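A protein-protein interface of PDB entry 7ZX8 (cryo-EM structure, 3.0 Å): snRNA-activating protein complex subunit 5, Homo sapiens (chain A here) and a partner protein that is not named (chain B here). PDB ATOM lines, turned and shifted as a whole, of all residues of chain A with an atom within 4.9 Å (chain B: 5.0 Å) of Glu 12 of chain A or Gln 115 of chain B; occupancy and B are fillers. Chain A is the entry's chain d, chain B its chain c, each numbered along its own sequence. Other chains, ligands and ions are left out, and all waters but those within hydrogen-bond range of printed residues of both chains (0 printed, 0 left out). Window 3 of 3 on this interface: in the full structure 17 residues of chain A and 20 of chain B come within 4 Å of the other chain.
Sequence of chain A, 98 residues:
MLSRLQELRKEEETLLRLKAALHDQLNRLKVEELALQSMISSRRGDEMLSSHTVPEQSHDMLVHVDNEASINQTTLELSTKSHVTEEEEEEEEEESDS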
ATOM      1  N   LEU A   5      -9.350  28.441   6.563  1.00  0.00           N
ATOM      2  CA  LEU A   5      -8.229  28.043   5.718  1.00  0.00           C
ATOM      3  C   LEU A   5      -6.965  28.807   6.088  1.00  0.00           C
ATOM      4  O   LEU A   5      -5.885  28.218   6.200  1.00  0.00           O
ATOM      5  CB  LEU A   5      -8.573  28.271   4.247  1.00  0.00           C
ATOM      6  CG  LEU A   5      -9.288  27.135   3.513  1.00  0.00           C
ATOM      7  CD1 LEU A   5      -8.350  25.958   3.299  1.00  0.00           C
ATOM      8  CD2 LEU A   5     -10.531  26.703   4.273  1.00  0.00           C
ATOM      9  N   LEU A   8      -5.649  27.699   9.502  1.00  0.00           N
ATOM     10  CA  LEU A   8      -4.991  26.403   9.393  1.00  0.00           C
ATOM     11  C   LEU A   8      -3.636  26.529   8.710  1.00  0.00           C
ATOM     12  O   LEU A   8      -2.661  25.901   9.134  1.00  0.00           O
ATOM     13  CB  LEU A   8      -5.886  25.425   8.631  1.00  0.00           C
ATOM     14  CG  LEU A   8      -7.201  25.050   9.316  1.00  0.00           C
ATOM     15  CD1 LEU A   8      -8.198  24.510   8.303  1.00  0.00           C
ATOM     16  CD2 LEU A   8      -6.960  24.038  10.425  1.00  0.00           C
ATOM     17  N   ARG A   9      -3.549  27.331   7.645  1.00  0.00           N
ATOM     18  CA  ARG A   9      -2.276  27.447   6.941  1.00  0.00           C
ATOM     19  C   ARG A   9      -1.239  28.174   7.788  1.00  0.00           C
ATOM     20  O   ARG A   9      -0.057  27.812   7.755  1.00  0.00           O
ATOM     21  CB  ARG A   9      -2.461  28.150   5.592  1.00  0.00           C
ATOM     22  CG  ARG A   9      -2.716  29.645   5.665  1.00  0.00           C
ATOM     23  CD  ARG A   9      -1.428  30.455   5.568  1.00  0.00           C
ATOM     24  NE  ARG A   9      -1.684  31.888   5.457  1.00  0.00           N
ATOM     25  CZ  ARG A   9      -0.748  32.826   5.564  1.00  0.00           C
ATOM     26  NH1 ARG A   9       0.516  32.489   5.784  1.00  0.00           N
ATOM     27  NH2 ARG A   9      -1.077  34.105   5.451  1.00  0.00           N
ATOM     28  N   LYS A  10      -1.645  29.193   8.551  1.00  0.00           N
ATOM     29  CA  LYS A  10      -0.681  29.850   9.428  1.00  0.00           C
ATOM     30  C   LYS A  10      -0.223  28.914  10.536  1.00  0.00           C
ATOM     31  O   LYS A  10       0.954  28.924  10.912  1.00  0.00           O
ATOM     32  CB  LYS A  10      -1.265  31.130  10.021  1.00  0.00           C
ATOM     33  CG  LYS A  10      -0.280  31.873  10.921  1.00  0.00           C
ATOM     34  CD  LYS A  10       0.989  32.264  10.177  1.00  0.00           C
ATOM     35  CE  LYS A  10       1.915  33.090  11.049  1.00  0.00           C
ATOM     36  NZ  LYS A  10       3.145  33.486  10.313  1.00  0.00           N
ATOM     37  N   GLU A  11      -1.134  28.105  11.085  1.00  0.00           N
ATOM     38  CA  GLU A  11      -0.702  27.086  12.037  1.00  0.00           C
ATOM     39  C   GLU A  11       0.259  26.102  11.384  1.00  0.00           C
ATOM     40  O   GLU A  11       1.220  25.648  12.019  1.00  0.00           O
ATOM     41  CB  GLU A  11      -1.915  26.349  12.605  1.00  0.00           C
ATOM     42  CG  GLU A  11      -2.781  27.201  13.519  1.00  0.00           C
ATOM     43  CD  GLU A  11      -3.994  26.453  14.036  1.00  0.00           C
ATOM     44  OE1 GLU A  11      -4.228  25.312  13.588  1.00  0.00           O
ATOM     45  OE2 GLU A  11      -4.714  27.008  14.892  1.00  0.00           O
ATOM     46  N   GLU A  12       0.014  25.766  10.116  1.00  0.00           N
ATOM     47  CA  GLU A  12       0.906  24.876   9.382  1.00  0.00           C
ATOM     48  C   GLU A  12       2.303  25.475   9.273  1.00  0.00           C
ATOM     49  O   GLU A  12       3.303  24.792   9.510  1.00  0.00           O
ATOM     50  CB  GLU A  12       0.316  24.596   7.998  1.00  0.00           C
ATOM     51  CG  GLU A  12       1.055  23.550   7.185  1.00  0.00           C
ATOM     52  CD  GLU A  12       0.683  23.584   5.716  1.00  0.00           C
ATOM     53  OE1 GLU A  12       1.447  24.172   4.921  1.00  0.00           O
ATOM     54  OE2 GLU A  12      -0.372  23.021   5.355  1.00  0.00           O
ATOM     55  N   GLU A  13       2.389  26.759   8.917  1.00  0.00           N
ATOM     56  CA  GLU A  13       3.696  27.413   8.844  1.00  0.00           C
ATOM     57  C   GLU A  13       4.352  27.493  10.218  1.00  0.00           C
ATOM     58  O   GLU A  13       5.568  27.307  10.344  1.00  0.00           O
ATOM     59  CB  GLU A  13       3.570  28.812   8.236  1.00  0.00           C
ATOM     60  CG  GLU A  13       2.748  28.897   6.958  1.00  0.00           C
ATOM     61  CD  GLU A  13       3.050  27.777   5.978  1.00  0.00           C
ATOM     62  OE1 GLU A  13       2.139  27.397   5.214  1.00  0.00           O
ATOM     63  OE2 GLU A  13       4.199  27.289   5.960  1.00  0.00           O
ATOM     64  N   THR A  14       3.565  27.784  11.256  1.00  0.00           N
ATOM     65  CA  THR A  14       4.093  27.817  12.616  1.00  0.00           C
ATOM     66  C   THR A  14       4.759  26.496  12.970  1.00  0.00           C
ATOM     67  O   THR A  14       5.915  26.458  13.416  1.00  0.00           O
ATOM     68  CB  THR A  14       2.958  28.114  13.600  1.00  0.00           C
ATOM     69  OG1 THR A  14       2.517  29.468  13.444  1.00  0.00           O
ATOM     70  CG2 THR A  14       3.406  27.875  15.038  1.00  0.00           C
ATOM     71  N   LEU A  15       4.036  25.397  12.770  1.00  0.00           N
ATOM     72  CA  LEU A  15       4.561  24.090  13.135  1.00  0.00           C
ATOM     73  C   LEU A  15       5.689  23.649  12.206  1.00  0.00           C
ATOM     74  O   LEU A  15       6.605  22.953  12.651  1.00  0.00           O
ATOM     75  CB  LEU A  15       3.405  23.084  13.195  1.00  0.00           C
ATOM     76  CG  LEU A  15       2.565  22.795  11.947  1.00  0.00           C
ATOM     77  CD1 LEU A  15       3.193  21.774  11.030  1.00  0.00           C
ATOM     78  CD2 LEU A  15       1.163  22.352  12.357  1.00  0.00           C
ATOM     79  N   LEU A  16       5.683  24.078  10.940  1.00  0.00           N
ATOM     80  CA  LEU A  16       6.841  23.835  10.080  1.00  0.00           C
ATOM     81  C   LEU A  16       8.085  24.540  10.604  1.00  0.00           C
ATOM     82  O   LEU A  16       9.177  23.965  10.598  1.00  0.00           O
ATOM     83  CB  LEU A  16       6.555  24.274   8.642  1.00  0.00           C
ATOM     84  CG  LEU A  16       5.965  23.249   7.667  1.00  0.00           C
ATOM     85  CD1 LEU A  16       6.948  22.110   7.443  1.00  0.00           C
ATOM     86  CD2 LEU A  16       4.647  22.702   8.151  1.00  0.00           C
ATOM     87  N   LEU B 108       1.079  17.851  12.128  1.00  0.00           N
ATOM     88  CA  LEU B 108       1.306  18.200  10.728  1.00  0.00           C
ATOM     89  C   LEU B 108       0.507  17.292   9.802  1.00  0.00           C
ATOM     90  O   LEU B 108      -0.081  17.755   8.819  1.00  0.00           O
ATOM     91  CB  LEU B 108       2.798  18.110  10.401  1.00  0.00           C
ATOM     92  CG  LEU B 108       3.196  18.240   8.925  1.00  0.00           C
ATOM     93  CD1 LEU B 108       2.575  19.470   8.274  1.00  0.00           C
ATOM     94  CD2 LEU B 108       4.711  18.270   8.782  1.00  0.00           C
ATOM     95  N   ASN B 111      -3.100  18.329   9.945  1.00  0.00           N
ATOM     96  CA  ASN B 111      -3.318  19.572   9.212  1.00  0.00           C
ATOM     97  C   ASN B 111      -3.297  19.337   7.707  1.00  0.00           C
ATOM     98  O   ASN B 111      -4.124  19.893   6.975  1.00  0.00           O
ATOM     99  CB  ASN B 111      -2.263  20.605   9.610  1.00  0.00           C
ATOM    100  CG  ASN B 111      -2.655  22.017   9.222  1.00  0.00           C
ATOM    101  OD1 ASN B 111      -3.532  22.223   8.384  1.00  0.00           O
ATOM    102  ND2 ASN B 111      -2.005  23.000   9.834  1.00  0.00           N
ATOM    103  N   ARG B 112      -2.365  18.513   7.224  1.00  0.00           N
ATOM    104  CA  ARG B 112      -2.315  18.221   5.796  1.00  0.00           C
ATOM    105  C   ARG B 112      -3.513  17.393   5.355  1.00  0.00           C
ATOM    106  O   ARG B 112      -3.993  17.555   4.229  1.00  0.00           O
ATOM    107  CB  ARG B 112      -1.010  17.501   5.447  1.00  0.00           C
ATOM    108  CG  ARG B 112       0.266  18.328   5.648  1.00  0.00           C
ATOM    109  CD  ARG B 112       0.067  19.808   5.345  1.00  0.00           C
ATOM    110  NE  ARG B 112       1.332  20.544   5.335  1.00  0.00           N
ATOM    111  CZ  ARG B 112       1.986  20.921   4.239  1.00  0.00           C
ATOM    112  NH1 ARG B 112       1.516  20.638   3.031  1.00  0.00           N
ATOM    113  NH2 ARG B 112       3.127  21.587   4.354  1.00  0.00           N
ATOM    114  N   GLU B 113      -4.015  16.509   6.219  1.00  0.00           N
ATOM    115  CA  GLU B 113      -5.248  15.794   5.905  1.00  0.00           C
ATOM    116  C   GLU B 113      -6.422  16.759   5.807  1.00  0.00           C
ATOM    117  O   GLU B 113      -7.281  16.620   4.930  1.00  0.00           O
ATOM    118  CB  GLU B 113      -5.516  14.722   6.963  1.00  0.00           C
ATOM    119  CG  GLU B 113      -6.801  13.932   6.749  1.00  0.00           C
ATOM    120  CD  GLU B 113      -6.965  13.448   5.321  1.00  0.00           C
ATOM    121  OE1 GLU B 113      -5.952  13.065   4.700  1.00  0.00           O
ATOM    122  OE2 GLU B 113      -8.109  13.452   4.820  1.00  0.00           O
ATOM    123  N   GLN B 114      -6.473  17.748   6.702  1.00  0.00           N
ATOM    124  CA  GLN B 114      -7.510  18.771   6.613  1.00  0.00           C
ATOM    125  C   GLN B 114      -7.389  19.557   5.313  1.00  0.00           C
ATOM    126  O   GLN B 114      -8.397  19.863   4.663  1.00  0.00           O
ATOM    127  CB  GLN B 114      -7.419  19.712   7.815  1.00  0.00           C
ATOM    128  CG  GLN B 114      -8.178  19.234   9.043  1.00  0.00           C
ATOM    129  CD  GLN B 114      -8.585  20.374   9.955  1.00  0.00           C
ATOM    130  OE1 GLN B 114      -9.168  21.363   9.511  1.00  0.00           O
ATOM    131  NE2 GLN B 114      -8.276  20.243  11.240  1.00  0.00           N
ATOM    132  N   GLN B 115      -6.160  19.898   4.922  1.00  0.00           N
ATOM    133  CA  GLN B 115      -5.957  20.604   3.660  1.00  0.00           C
ATOM    134  C   GLN B 115      -6.407  19.756   2.477  1.00  0.00           C
ATOM    135  O   GLN B 115      -7.027  20.266   1.539  1.00  0.00           O
ATOM    136  CB  GLN B 115      -4.488  21.001   3.501  1.00  0.00           C
ATOM    137  CG  GLN B 115      -3.956  21.970   4.556  1.00  0.00           C
ATOM    138  CD  GLN B 115      -4.968  23.022   4.965  1.00  0.00           C
ATOM    139  OE1 GLN B 115      -5.486  23.000   6.082  1.00  0.00           O
ATOM    140  NE2 GLN B 115      -5.253  23.954   4.062  1.00  0.00           N
ATOM    141  N   GLU B 116      -6.096  18.460   2.495  1.00  0.00           N
ATOM    142  CA  GLU B 116      -6.541  17.584   1.414  1.00  0.00           C
ATOM    143  C   GLU B 116      -8.061  17.495   1.378  1.00  0.00           C
ATOM    144  O   GLU B 116      -8.668  17.476   0.299  1.00  0.00           O
ATOM    145  CB  GLU B 116      -5.923  16.195   1.577  1.00  0.00           C
ATOM    146  CG  GLU B 116      -5.864  15.390   0.287  1.00  0.00           C
ATOM    147  CD  GLU B 116      -7.063  14.479   0.113  1.00  0.00           C
ATOM    148  OE1 GLU B 116      -7.700  14.532  -0.961  1.00  0.00           O
ATOM    149  OE2 GLU B 116      -7.368  13.708   1.047  1.00  0.00           O
ATOM    150  N   GLU B 117      -8.694  17.439   2.551  1.00  0.00           N
ATOM    151  CA  GLU B 117     -10.151  17.443   2.607  1.00  0.00           C
ATOM    152  C   GLU B 117     -10.713  18.721   1.995  1.00  0.00           C
ATOM    153  O   GLU B 117     -11.689  18.683   1.238  1.00  0.00           O
ATOM    154  CB  GLU B 117     -10.617  17.288   4.055  1.00  0.00           C
ATOM    155  CG  GLU B 117     -10.320  15.916   4.651  1.00  0.00           C
ATOM    156  CD  GLU B 117     -10.330  15.914   6.168  1.00  0.00           C
ATOM    157  OE1 GLU B 117     -10.448  17.001   6.771  1.00  0.00           O
ATOM    158  OE2 GLU B 117     -10.218  14.819   6.761  1.00  0.00           O
ATOM    159  N   LEU B 118     -10.100  19.864   2.305  1.00  0.00           N
ATOM    160  CA  LEU B 118     -10.562  21.126   1.736  1.00  0.00           C
ATOM    161  C   LEU B 118     -10.374  21.158   0.221  1.00  0.00           C
ATOM    162  O   LEU B 118     -11.260  21.613  -0.512  1.00  0.00           O
ATOM    163  CB  LEU B 118      -9.832  22.293   2.402  1.00  0.00           C
ATOM    164  CG  LEU B 118     -10.059  22.393   3.916  1.00  0.00           C
ATOM    165  CD1 LEU B 118      -8.843  22.982   4.626  1.00  0.00           C
ATOM    166  CD2 LEU B 118     -11.314  23.200   4.220  1.00  0.00           C
ATOM    167  N   MET B 119      -9.229  20.677  -0.269  1.00  0.00           N
ATOM    168  CA  MET B 119      -9.010  20.621  -1.714  1.00  0.00           C
ATOM    169  C   MET B 119     -10.057  19.752  -2.398  1.00  0.00           C
ATOM    170  O   MET B 119     -10.621  20.140  -3.428  1.00  0.00           O
ATOM    171  CB  MET B 119      -7.602  20.102  -2.026  1.00  0.00           C
ATOM    172  CG  MET B 119      -6.423  20.913  -1.476  1.00  0.00           C
ATOM    173  SD  MET B 119      -6.644  22.713  -1.433  1.00  0.00           S
ATOM    174  CE  MET B 119      -7.415  23.018   0.151  1.00  0.00           C
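N of Glu 12 of chain A sits close to ND2 of Asn 111 of chain B, at 3.4 Å.
The guanidinium group of Arg 112 of chain B lies within salt-bridge range of the side-chain carboxylate of Glu 12 of chain A (3.0 Å).
ND2 of Asn 111 of chain B sits at hydrogen-bond distance from O of Leu 8 of chain A (3.1 Å).
The side-chain amide oxygen of Gln 115 of chain B sits close to the side-chain amide oxygen of Asn 111 of chain B (3.1 Å).
Among the printed residues, merely in contact across the chains: Leu 5 of chain A with Gln 115 of chain B, Leu 5 of chain A with Leu 118 of chain B, Leu 8 of chain A with Gln 114 of chain B, Leu 8 of chain A with Gln 115 of chain B, Glu 12 of chain A with Gln 115 of chain B, Leu 15 of chain A with Leu 108 of chain B and Leu 16 of chain A with Leu 108 of chain B.
Printed residues of chain B within 4 Å of Leu 8 of chain A: Asn 111 (3.1 Å), Gln 114 (3.5 Å) and Gln 115 (3.5 Å).
Lys 10 of chain A touches none of the printed residues of chain B.
Glu 12 of chain A touches just these residues of chain B: Asn 111, Arg 112 and Gln 115.
Of the printed residues of chain A, Asn 111 of chain B touches Leu 8 and Glu 12.
Gln 115 of chain B touches just these residues of chain A: Leu 5, Leu 8 and Glu 12.
Glu 116 of chain B touches none of the printed residues of chain A.
The nearest printed residue of chain A that does not touch Gln 115 of chain B is Arg 9 of chain A (5.0 Å).
Among the printed residues, Asp or Glu carboxylates within 4 Å of a Lys or Arg side-chain nitrogen of the other chain: Glu 12 of chain A with Arg 112 of chain B (3.0 Å).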
